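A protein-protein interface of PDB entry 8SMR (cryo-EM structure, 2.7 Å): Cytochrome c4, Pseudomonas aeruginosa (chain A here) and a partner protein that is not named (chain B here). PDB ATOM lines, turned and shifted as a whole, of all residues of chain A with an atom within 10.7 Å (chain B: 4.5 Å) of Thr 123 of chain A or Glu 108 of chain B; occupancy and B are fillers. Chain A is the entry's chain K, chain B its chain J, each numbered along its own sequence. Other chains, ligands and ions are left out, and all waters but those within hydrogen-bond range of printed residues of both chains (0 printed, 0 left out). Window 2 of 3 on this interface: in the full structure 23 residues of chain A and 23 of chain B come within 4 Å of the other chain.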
ATOM      1  N   ALA A   1     -13.202  13.179  32.430  1.00  0.00           N
ATOM      2  CA  ALA A   1     -14.564  13.584  32.106  1.00  0.00           C
ATOM      3  C   ALA A   1     -15.039  14.677  33.055  1.00  0.00           C
ATOM      4  O   ALA A   1     -14.569  14.774  34.190  1.00  0.00           O
ATOM      5  CB  ALA A   1     -15.499  12.388  32.163  1.00  0.00           C
ATOM      6  N   GLY A  34     -27.910  19.202  25.097  1.00  0.00           N
ATOM      7  CA  GLY A  34     -27.858  17.966  24.351  1.00  0.00           C
ATOM      8  C   GLY A  34     -26.727  17.862  23.357  1.00  0.00           C
ATOM      9  O   GLY A  34     -26.620  16.838  22.674  1.00  0.00           O
ATOM     10  N   GLN A  35     -25.878  18.880  23.249  1.00  0.00           N
ATOM     11  CA  GLN A  35     -24.748  18.815  22.338  1.00  0.00           C
ATOM     12  C   GLN A  35     -23.686  17.869  22.883  1.00  0.00           C
ATOM     13  O   GLN A  35     -23.504  17.736  24.096  1.00  0.00           O
ATOM     14  CB  GLN A  35     -24.155  20.209  22.122  1.00  0.00           C
ATOM     15  CG  GLN A  35     -23.066  20.276  21.062  1.00  0.00           C
ATOM     16  CD  GLN A  35     -23.508  19.702  19.733  1.00  0.00           C
ATOM     17  OE1 GLN A  35     -23.395  18.500  19.499  1.00  0.00           O
ATOM     18  NE2 GLN A  35     -24.013  20.558  18.855  1.00  0.00           N
ATOM     19  N   GLY A  36     -22.986  17.203  21.971  1.00  0.00           N
ATOM     20  CA  GLY A  36     -21.957  16.260  22.360  1.00  0.00           C
ATOM     21  C   GLY A  36     -20.924  16.887  23.270  1.00  0.00           C
ATOM     22  O   GLY A  36     -20.425  17.981  22.989  1.00  0.00           O
ATOM     23  N   GLU A  37     -20.593  16.205  24.367  1.00  0.00           N
ATOM     24  CA  GLU A  37     -19.638  16.764  25.318  1.00  0.00           C
ATOM     25  C   GLU A  37     -18.277  16.968  24.666  1.00  0.00           C
ATOM     26  O   GLU A  37     -17.617  17.988  24.895  1.00  0.00           O
ATOM     27  CB  GLU A  37     -19.520  15.855  26.540  1.00  0.00           C
ATOM     28  CG  GLU A  37     -18.231  16.034  27.327  1.00  0.00           C
ATOM     29  CD  GLU A  37     -18.362  15.593  28.772  1.00  0.00           C
ATOM     30  OE1 GLU A  37     -19.333  14.877  29.093  1.00  0.00           O
ATOM     31  OE2 GLU A  37     -17.491  15.962  29.588  1.00  0.00           O
ATOM     32  N   ARG A  38     -17.840  16.011  23.845  1.00  0.00           N
ATOM     33  CA  ARG A  38     -16.572  16.170  23.143  1.00  0.00           C
ATOM     34  C   ARG A  38     -16.603  17.394  22.238  1.00  0.00           C
ATOM     35  O   ARG A  38     -15.664  18.200  22.231  1.00  0.00           O
ATOM     36  CB  ARG A  38     -16.260  14.911  22.334  1.00  0.00           C
ATOM     37  CG  ARG A  38     -15.099  15.073  21.366  1.00  0.00           C
ATOM     38  CD  ARG A  38     -14.689  13.750  20.749  1.00  0.00           C
ATOM     39  NE  ARG A  38     -13.649  13.919  19.743  1.00  0.00           N
ATOM     40  CZ  ARG A  38     -13.152  12.937  19.003  1.00  0.00           C
ATOM     41  NH1 ARG A  38     -13.575  11.691  19.133  1.00  0.00           N
ATOM     42  NH2 ARG A  38     -12.207  13.213  18.110  1.00  0.00           N
ATOM     43  N   TYR A  39     -17.678  17.551  21.463  1.00  0.00           N
ATOM     44  CA  TYR A  39     -17.774  18.699  20.568  1.00  0.00           C
ATOM     45  C   TYR A  39     -17.843  20.006  21.347  1.00  0.00           C
ATOM     46  O   TYR A  39     -17.204  20.993  20.968  1.00  0.00           O
ATOM     47  CB  TYR A  39     -18.995  18.565  19.659  1.00  0.00           C
ATOM     48  CG  TYR A  39     -19.222  19.790  18.804  1.00  0.00           C
ATOM     49  CD1 TYR A  39     -18.524  19.969  17.620  1.00  0.00           C
ATOM     50  CD2 TYR A  39     -20.119  20.777  19.191  1.00  0.00           C
ATOM     51  CE1 TYR A  39     -18.718  21.085  16.840  1.00  0.00           C
ATOM     52  CE2 TYR A  39     -20.320  21.900  18.414  1.00  0.00           C
ATOM     53  CZ  TYR A  39     -19.615  22.048  17.240  1.00  0.00           C
ATOM     54  OH  TYR A  39     -19.806  23.161  16.457  1.00  0.00           O
ATOM     55  N   LEU A  40     -18.629  20.041  22.425  1.00  0.00           N
ATOM     56  CA  LEU A  40     -18.719  21.256  23.228  1.00  0.00           C
ATOM     57  C   LEU A  40     -17.358  21.636  23.793  1.00  0.00           C
ATOM     58  O   LEU A  40     -16.962  22.807  23.752  1.00  0.00           O
ATOM     59  CB  LEU A  40     -19.725  21.061  24.362  1.00  0.00           C
ATOM     60  CG  LEU A  40     -21.209  21.173  24.016  1.00  0.00           C
ATOM     61  CD1 LEU A  40     -22.052  20.768  25.213  1.00  0.00           C
ATOM     62  CD2 LEU A  40     -21.564  22.579  23.565  1.00  0.00           C
ATOM     63  N   LEU A  41     -16.629  20.654  24.327  1.00  0.00           N
ATOM     64  CA  LEU A  41     -15.313  20.932  24.886  1.00  0.00           C
ATOM     65  C   LEU A  41     -14.349  21.402  23.806  1.00  0.00           C
ATOM     66  O   LEU A  41     -13.564  22.331  24.030  1.00  0.00           O
ATOM     67  CB  LEU A  41     -14.776  19.683  25.587  1.00  0.00           C
ATOM     68  CG  LEU A  41     -13.613  19.871  26.564  1.00  0.00           C
ATOM     69  CD1 LEU A  41     -13.970  20.875  27.650  1.00  0.00           C
ATOM     70  CD2 LEU A  41     -13.223  18.536  27.179  1.00  0.00           C
ATOM     71  N   LYS A  42     -14.396  20.781  22.624  1.00  0.00           N
ATOM     72  CA  LYS A  42     -13.532  21.217  21.534  1.00  0.00           C
ATOM     73  C   LYS A  42     -13.840  22.652  21.132  1.00  0.00           C
ATOM     74  O   LYS A  42     -12.924  23.449  20.911  1.00  0.00           O
ATOM     75  CB  LYS A  42     -13.684  20.284  20.332  1.00  0.00           C
ATOM     76  CG  LYS A  42     -12.867  20.705  19.117  1.00  0.00           C
ATOM     77  CD  LYS A  42     -13.219  19.889  17.891  1.00  0.00           C
ATOM     78  CE  LYS A  42     -12.273  20.191  16.742  1.00  0.00           C
ATOM     79  NZ  LYS A  42     -12.300  21.628  16.357  1.00  0.00           N
ATOM     80  N   ALA A  77     -24.186  18.746  27.802  1.00  0.00           N
ATOM     81  CA  ALA A  77     -24.433  17.477  27.130  1.00  0.00           C
ATOM     82  C   ALA A  77     -25.457  16.625  27.865  1.00  0.00           C
ATOM     83  O   ALA A  77     -26.037  15.717  27.262  1.00  0.00           O
ATOM     84  CB  ALA A  77     -23.125  16.698  26.986  1.00  0.00           C
ATOM     85  N   GLY A 112     -24.783  10.929   7.510  1.00  0.00           N
ATOM     86  CA  GLY A 112     -23.696  10.041   7.868  1.00  0.00           C
ATOM     87  C   GLY A 112     -22.985  10.469   9.132  1.00  0.00           C
ATOM     88  O   GLY A 112     -23.034   9.774  10.150  1.00  0.00           O
ATOM     89  N   CYS A 113     -22.318  11.622   9.079  1.00  0.00           N
ATOM     90  CA  CYS A 113     -21.587  12.117  10.238  1.00  0.00           C
ATOM     91  C   CYS A 113     -22.522  12.650  11.314  1.00  0.00           C
ATOM     92  O   CYS A 113     -22.316  12.376  12.500  1.00  0.00           O
ATOM     93  CB  CYS A 113     -20.614  13.206   9.803  1.00  0.00           C
ATOM     94  SG  CYS A 113     -19.670  12.792   8.314  1.00  0.00           S
ATOM     95  N   SER A 115     -26.309  12.208  12.630  1.00  0.00           N
ATOM     96  CA  SER A 115     -27.229  11.086  12.493  1.00  0.00           C
ATOM     97  C   SER A 115     -28.375  11.429  11.549  1.00  0.00           C
ATOM     98  O   SER A 115     -28.597  12.605  11.239  1.00  0.00           O
ATOM     99  CB  SER A 115     -27.780  10.686  13.860  1.00  0.00           C
ATOM    100  OG  SER A 115     -26.782  10.068  14.648  1.00  0.00           O
ATOM    101  N   VAL A 119     -28.736  13.915  15.624  1.00  0.00           N
ATOM    102  CA  VAL A 119     -28.155  13.917  16.966  1.00  0.00           C
ATOM    103  C   VAL A 119     -26.637  13.927  16.959  1.00  0.00           C
ATOM    104  O   VAL A 119     -26.025  14.042  18.028  1.00  0.00           O
ATOM    105  CB  VAL A 119     -28.625  12.700  17.786  1.00  0.00           C
ATOM    106  CG1 VAL A 119     -30.109  12.804  18.085  1.00  0.00           C
ATOM    107  CG2 VAL A 119     -28.316  11.399  17.056  1.00  0.00           C
ATOM    108  N   GLY A 120     -26.010  13.806  15.796  1.00  0.00           N
ATOM    109  CA  GLY A 120     -24.568  13.749  15.739  1.00  0.00           C
ATOM    110  C   GLY A 120     -24.033  12.445  16.296  1.00  0.00           C
ATOM    111  O   GLY A 120     -24.770  11.502  16.601  1.00  0.00           O
ATOM    112  N   ILE A 121     -22.712  12.398  16.425  1.00  0.00           N
ATOM    113  CA  ILE A 121     -22.007  11.279  17.041  1.00  0.00           C
ATOM    114  C   ILE A 121     -21.179  11.876  18.170  1.00  0.00           C
ATOM    115  O   ILE A 121     -20.147  12.510  17.925  1.00  0.00           O
ATOM    116  CB  ILE A 121     -21.130  10.512  16.046  1.00  0.00           C
ATOM    117  CG1 ILE A 121     -21.933  10.178  14.787  1.00  0.00           C
ATOM    118  CG2 ILE A 121     -20.597   9.237  16.682  1.00  0.00           C
ATOM    119  CD1 ILE A 121     -21.182   9.339  13.779  1.00  0.00           C
ATOM    120  N   ALA A 122     -21.628  11.678  19.410  1.00  0.00           N
ATOM    121  CA  ALA A 122     -20.981  12.330  20.543  1.00  0.00           C
ATOM    122  C   ALA A 122     -19.532  11.889  20.689  1.00  0.00           C
ATOM    123  O   ALA A 122     -18.643  12.719  20.911  1.00  0.00           O
ATOM    124  CB  ALA A 122     -21.762  12.040  21.825  1.00  0.00           C
ATOM    125  N   THR A 123     -19.271  10.585  20.569  1.00  0.00           N
ATOM    126  CA  THR A 123     -17.907  10.092  20.737  1.00  0.00           C
ATOM    127  C   THR A 123     -16.989  10.625  19.647  1.00  0.00           C
ATOM    128  O   THR A 123     -15.839  10.991  19.916  1.00  0.00           O
ATOM    129  CB  THR A 123     -17.898   8.563  20.744  1.00  0.00           C
ATOM    130  OG1 THR A 123     -18.543   8.071  19.563  1.00  0.00           O
ATOM    131  CG2 THR A 123     -18.615   8.032  21.974  1.00  0.00           C
ATOM    132  N   ALA A 124     -17.475  10.676  18.405  1.00  0.00           N
ATOM    133  CA  ALA A 124     -16.655  11.142  17.293  1.00  0.00           C
ATOM    134  C   ALA A 124     -16.506  12.655  17.262  1.00  0.00           C
ATOM    135  O   ALA A 124     -15.685  13.161  16.490  1.00  0.00           O
ATOM    136  CB  ALA A 124     -17.249  10.665  15.968  1.00  0.00           C
ATOM    137  N   GLY A 125     -17.266  13.383  18.075  1.00  0.00           N
ATOM    138  CA  GLY A 125     -17.224  14.827  18.046  1.00  0.00           C
ATOM    139  C   GLY A 125     -18.067  15.464  16.966  1.00  0.00           C
ATOM    140  O   GLY A 125     -17.995  16.684  16.790  1.00  0.00           O
ATOM    141  N   PHE A 126     -18.860  14.684  16.241  1.00  0.00           N
ATOM    142  CA  PHE A 126     -19.755  15.250  15.243  1.00  0.00           C
ATOM    143  C   PHE A 126     -20.926  15.922  15.953  1.00  0.00           C
ATOM    144  O   PHE A 126     -21.662  15.248  16.683  1.00  0.00           O
ATOM    145  CB  PHE A 126     -20.254  14.165  14.296  1.00  0.00           C
ATOM    146  CG  PHE A 126     -19.160  13.493  13.505  1.00  0.00           C
ATOM    147  CD1 PHE A 126     -17.945  14.122  13.284  1.00  0.00           C
ATOM    148  CD2 PHE A 126     -19.349  12.224  12.985  1.00  0.00           C
ATOM    149  CE1 PHE A 126     -16.948  13.501  12.560  1.00  0.00           C
ATOM    150  CE2 PHE A 126     -18.355  11.599  12.258  1.00  0.00           C
ATOM    151  CZ  PHE A 126     -17.153  12.238  12.048  1.00  0.00           C
ATOM    152  N   PRO A 127     -21.134  17.224  15.777  1.00  0.00           N
ATOM    153  CA  PRO A 127     -22.093  17.933  16.630  1.00  0.00           C
ATOM    154  C   PRO A 127     -23.532  17.512  16.387  1.00  0.00           C
ATOM    155  O   PRO A 127     -23.932  17.174  15.271  1.00  0.00           O
ATOM    156  CB  PRO A 127     -21.885  19.404  16.254  1.00  0.00           C
ATOM    157  CG  PRO A 127     -21.271  19.380  14.913  1.00  0.00           C
ATOM    158  CD  PRO A 127     -20.461  18.132  14.833  1.00  0.00           C
ATOM    159  N   HIS A 128     -24.308  17.537  17.466  1.00  0.00           N
ATOM    160  CA  HIS A 128     -25.759  17.487  17.354  1.00  0.00           C
ATOM    161  C   HIS A 128     -26.246  18.669  16.527  1.00  0.00           C
ATOM    162  O   HIS A 128     -25.835  19.811  16.754  1.00  0.00           O
ATOM    163  CB  HIS A 128     -26.379  17.507  18.753  1.00  0.00           C
ATOM    164  CG  HIS A 128     -27.874  17.414  18.766  1.00  0.00           C
ATOM    165  ND1 HIS A 128     -28.548  16.421  19.444  1.00  0.00           N
ATOM    166  CD2 HIS A 128     -28.824  18.201  18.211  1.00  0.00           C
ATOM    167  CE1 HIS A 128     -29.849  16.592  19.292  1.00  0.00           C
ATOM    168  NE2 HIS A 128     -30.043  17.666  18.548  1.00  0.00           N
ATOM    169  N   TYR B 107     -17.006   0.006  20.781  1.00  0.00           N
ATOM    170  CA  TYR B 107     -16.948   0.406  22.179  1.00  0.00           C
ATOM    171  C   TYR B 107     -16.135   1.683  22.316  1.00  0.00           C
ATOM    172  O   TYR B 107     -15.179   1.911  21.574  1.00  0.00           O
ATOM    173  CB  TYR B 107     -16.340  -0.694  23.058  1.00  0.00           C
ATOM    174  CG  TYR B 107     -14.921  -1.067  22.697  1.00  0.00           C
ATOM    175  CD1 TYR B 107     -13.843  -0.407  23.270  1.00  0.00           C
ATOM    176  CD2 TYR B 107     -14.657  -2.081  21.787  1.00  0.00           C
ATOM    177  CE1 TYR B 107     -12.545  -0.743  22.946  1.00  0.00           C
ATOM    178  CE2 TYR B 107     -13.361  -2.424  21.456  1.00  0.00           C
ATOM    179  CZ  TYR B 107     -12.309  -1.752  22.041  1.00  0.00           C
ATOM    180  OH  TYR B 107     -11.017  -2.090  21.713  1.00  0.00           O
ATOM    181  N   GLU B 108     -16.508   2.506  23.293  1.00  0.00           N
ATOM    182  CA  GLU B 108     -15.857   3.796  23.467  1.00  0.00           C
ATOM    183  C   GLU B 108     -14.367   3.618  23.725  1.00  0.00           C
ATOM    184  O   GLU B 108     -13.956   2.774  24.527  1.00  0.00           O
ATOM    185  CB  GLU B 108     -16.509   4.563  24.617  1.00  0.00           C
ATOM    186  CG  GLU B 108     -17.973   4.883  24.376  1.00  0.00           C
ATOM    187  CD  GLU B 108     -18.519   5.900  25.356  1.00  0.00           C
ATOM    188  OE1 GLU B 108     -19.381   5.529  26.177  1.00  0.00           O
ATOM    189  OE2 GLU B 108     -18.089   7.070  25.303  1.00  0.00           O
ATOM    190  N   ASP B 109     -13.559   4.422  23.037  1.00  0.00           N
ATOM    191  CA  ASP B 109     -12.102   4.350  23.149  1.00  0.00           C
ATOM    192  C   ASP B 109     -11.546   5.748  22.933  1.00  0.00           C
ATOM    193  O   ASP B 109     -11.282   6.160  21.796  1.00  0.00           O
ATOM    194  CB  ASP B 109     -11.509   3.367  22.141  1.00  0.00           C
ATOM    195  CG  ASP B 109     -10.037   3.101  22.384  1.00  0.00           C
ATOM    196  OD1 ASP B 109      -9.487   3.637  23.368  1.00  0.00           O
ATOM    197  OD2 ASP B 109      -9.428   2.356  21.590  1.00  0.00           O
ATOM    198  N   PRO B 110     -11.347   6.514  24.010  1.00  0.00           N
ATOM    199  CA  PRO B 110     -10.919   7.913  23.835  1.00  0.00           C
ATOM    200  C   PRO B 110      -9.613   8.060  23.078  1.00  0.00           C
ATOM    201  O   PRO B 110      -9.381   9.107  22.459  1.00  0.00           O
ATOM    202  CB  PRO B 110     -10.795   8.423  25.277  1.00  0.00           C
ATOM    203  CG  PRO B 110     -11.659   7.519  26.084  1.00  0.00           C
ATOM    204  CD  PRO B 110     -11.574   6.179  25.426  1.00  0.00           C
ATOM    205  N   TRP B 114     -12.135   8.876  16.544  1.00  0.00           N
ATOM    206  CA  TRP B 114     -13.571   9.063  16.694  1.00  0.00           C
ATOM    207  C   TRP B 114     -14.080   8.587  18.047  1.00  0.00           C
ATOM    208  O   TRP B 114     -15.292   8.421  18.224  1.00  0.00           O
ATOM    209  CB  TRP B 114     -14.313   8.352  15.563  1.00  0.00           C
ATOM    210  CG  TRP B 114     -13.782   8.711  14.215  1.00  0.00           C
ATOM    211  CD1 TRP B 114     -13.386   7.854  13.233  1.00  0.00           C
ATOM    212  CD2 TRP B 114     -13.579  10.031  13.702  1.00  0.00           C
ATOM    213  NE1 TRP B 114     -12.950   8.559  12.139  1.00  0.00           N
ATOM    214  CE2 TRP B 114     -13.060   9.899  12.402  1.00  0.00           C
ATOM    215  CE3 TRP B 114     -13.789  11.314  14.216  1.00  0.00           C
ATOM    216  CZ2 TRP B 114     -12.747  10.999  11.609  1.00  0.00           C
ATOM    217  CZ3 TRP B 114     -13.478  12.403  13.428  1.00  0.00           C
ATOM    218  CH2 TRP B 114     -12.963  12.240  12.139  1.00  0.00           C
ATOM    219  N   GLY B 115     -13.182   8.361  19.003  1.00  0.00           N
ATOM    220  CA  GLY B 115     -13.591   8.010  20.344  1.00  0.00           C
ATOM    221  C   GLY B 115     -14.091   6.598  20.510  1.00  0.00           C
ATOM    222  O   GLY B 115     -14.584   6.256  21.588  1.00  0.00           O
ATOM    223  N   VAL B 116     -13.982   5.761  19.478  1.00  0.00           N
ATOM    224  CA  VAL B 116     -14.463   4.389  19.534  1.00  0.00           C
ATOM    225  C   VAL B 116     -13.449   3.474  18.866  1.00  0.00           C
ATOM    226  O   VAL B 116     -12.653   3.890  18.022  1.00  0.00           O
ATOM    227  CB  VAL B 116     -15.845   4.219  18.863  1.00  0.00           C
ATOM    228  CG1 VAL B 116     -16.907   4.994  19.626  1.00  0.00           C
ATOM    229  CG2 VAL B 116     -15.791   4.657  17.408  1.00  0.00           C
ATOM    230  N   ARG B 136     -24.300   3.627  24.643  1.00  0.00           N
ATOM    231  CA  ARG B 136     -22.874   3.662  24.948  1.00  0.00           C
ATOM    232  C   ARG B 136     -22.398   2.262  25.313  1.00  0.00           C
ATOM    233  O   ARG B 136     -22.875   1.669  26.286  1.00  0.00           O
ATOM    234  CB  ARG B 136     -22.603   4.646  26.080  1.00  0.00           C
ATOM    235  CG  ARG B 136     -22.998   6.080  25.753  1.00  0.00           C
ATOM    236  CD  ARG B 136     -22.590   7.054  26.851  1.00  0.00           C
ATOM    237  NE  ARG B 136     -21.198   6.884  27.255  1.00  0.00           N
ATOM    238  CZ  ARG B 136     -20.791   6.490  28.456  1.00  0.00           C
ATOM    239  NH1 ARG B 136     -21.647   6.217  29.428  1.00  0.00           N
ATOM    240  NH2 ARG B 136     -19.487   6.368  28.689  1.00  0.00           N
ATOM    241  N   GLN B 137     -21.457   1.734  24.536  1.00  0.00           N
ATOM    242  CA  GLN B 137     -20.855   0.431  24.785  1.00  0.00           C
ATOM    243  C   GLN B 137     -19.400   0.632  25.183  1.00  0.00           C
ATOM    244  O   GLN B 137     -18.684   1.417  24.553  1.00  0.00           O
ATOM    245  CB  GLN B 137     -20.958  -0.466  23.550  1.00  0.00           C
ATOM    246  CG  GLN B 137     -20.434  -1.876  23.761  1.00  0.00           C
ATOM    247  CD  GLN B 137     -20.932  -2.850  22.712  1.00  0.00           C
ATOM    248  OE1 GLN B 137     -21.769  -3.705  22.992  1.00  0.00           O
ATOM    249  NE2 GLN B 137     -20.416  -2.725  21.497  1.00  0.00           N
ATOM    250  N   VAL B 138     -18.971  -0.066  26.233  1.00  0.00           N
ATOM    251  CA  VAL B 138     -17.654   0.131  26.818  1.00  0.00           C
ATOM    252  C   VAL B 138     -17.025  -1.221  27.123  1.00  0.00           C
ATOM    253  O   VAL B 138     -17.703  -2.246  27.222  1.00  0.00           O
ATOM    254  CB  VAL B 138     -17.717   0.988  28.100  1.00  0.00           C
ATOM    255  CG1 VAL B 138     -18.150   2.404  27.767  1.00  0.00           C
ATOM    256  CG2 VAL B 138     -18.664   0.362  29.116  1.00  0.00           C
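Printed residues of chain A that touch a printed residue of chain B: Arg 38, Thr 123, Ala 124 and Phe 126.
Hydrophobic or aromatic side chains of chain B that line the printed part of chain A: Trp 114 and Val 116.
Among the printed residues, 8 pairs touch across the chains.
Among the printed residues, no Asp or Glu carboxylate lies within 4 Å of a Lys or Arg side-chain nitrogen of the other chain.
The guanidinium group (NH1) of Arg 38 of chain A is in hydrogen-bond range of the backbone carbonyl oxygen (O) of Thr 123 of chain A.
The backbone NH (N) of Glu 108 of chain B lies within hydrogen-bond range of the backbone carbonyl oxygen (O) of Gln 137 of chain B, at 2.7 Å.
The backbone NH (N) of Asp 109 of chain B sits at hydrogen-bond distance from the backbone carbonyl oxygen (O) of Gly 115 of chain B, at 2.6 Å.
The backbone NH (N) of Phe 126 of chain A lies within hydrogen-bond range of the backbone carbonyl oxygen (O) of Ile 121 of chain A, 3.0 Å away.
The side-chain carboxylate (OE1) of Glu 108 of chain B lies within salt-bridge range of the guanidinium group (NE) of Arg 136 of chain B, at 2.5 Å.
Printed residues of chain B within 4 Å of Arg 38 of chain A: Trp 114 (3.3 Å) and Gly 115 (3.4 Å).
Leu 40 of chain A touches none of the printed residues of chain B.
Thr 123 of chain A touches just these residues of chain B: Glu 108, Trp 114, Gly 115 and Val 116.
Of the printed residues of chain B, Ala 124 of chain A touches Trp 114 (3.1 Å).
Of the printed residues of chain B, Phe 126 of chain A touches Trp 114 (3.7 Å).
Pro 127 of chain A touches none of the printed residues of chain B.
No residue of chain A comes within 4 Å of Tyr 107 of chain B.
Glu 108 of chain B touches one residue of chain A.
Of the printed residues of chain A, Trp 114 of chain B touches Arg 38 (3.3 Å), Thr 123 (3.1 Å), Ala 124 (3.1 Å) and Phe 126 (3.7 Å).
Of chain A, only Arg 38 and Thr 123 come within 4 Å of Gly 115 of chain B.
Of the printed residues of chain A, Val 116 of chain B touches Thr 123.
Val 138 of chain B touches none of the printed residues of chain A.
The nearest printed residue of chain B that does not touch Thr 123 of chain A is Arg 136 of chain B (6.0 Å).
The nearest residue of chain A that does not touch Glu 108 of chain B is Ala 122 of chain A (6.8 Å).
Arg 38 of chain A touches Trp 114 of chain B (NH1 to C, 3.3 Å).
Glu 108 of chain B touches Thr 123 of chain A (OE2 to CG2, 3.5 Å).
Thr 123 of chain A touches Gly 115 of chain B.
Val 116 of chain B touches Thr 123 of chain A (CG1 to OG1, 3.5 Å).
Phe 126 of chain A touches Trp 114 of chain B (CE1 to CZ3, 3.7 Å).
The guanidinium group of Arg 38 of chain A lies close to the backbone NH of Gly 115 of chain B.
The backbone NH (N) of Ala 124 of chain A is in hydrogen-bond range of the backbone carbonyl oxygen (O) of Trp 114 of chain B.
The backbone carbonyl oxygen (O) of Trp 114 of chain B sits close to the backbone carbonyl oxygen (O) of Thr 123 of chain A (3.1 Å).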
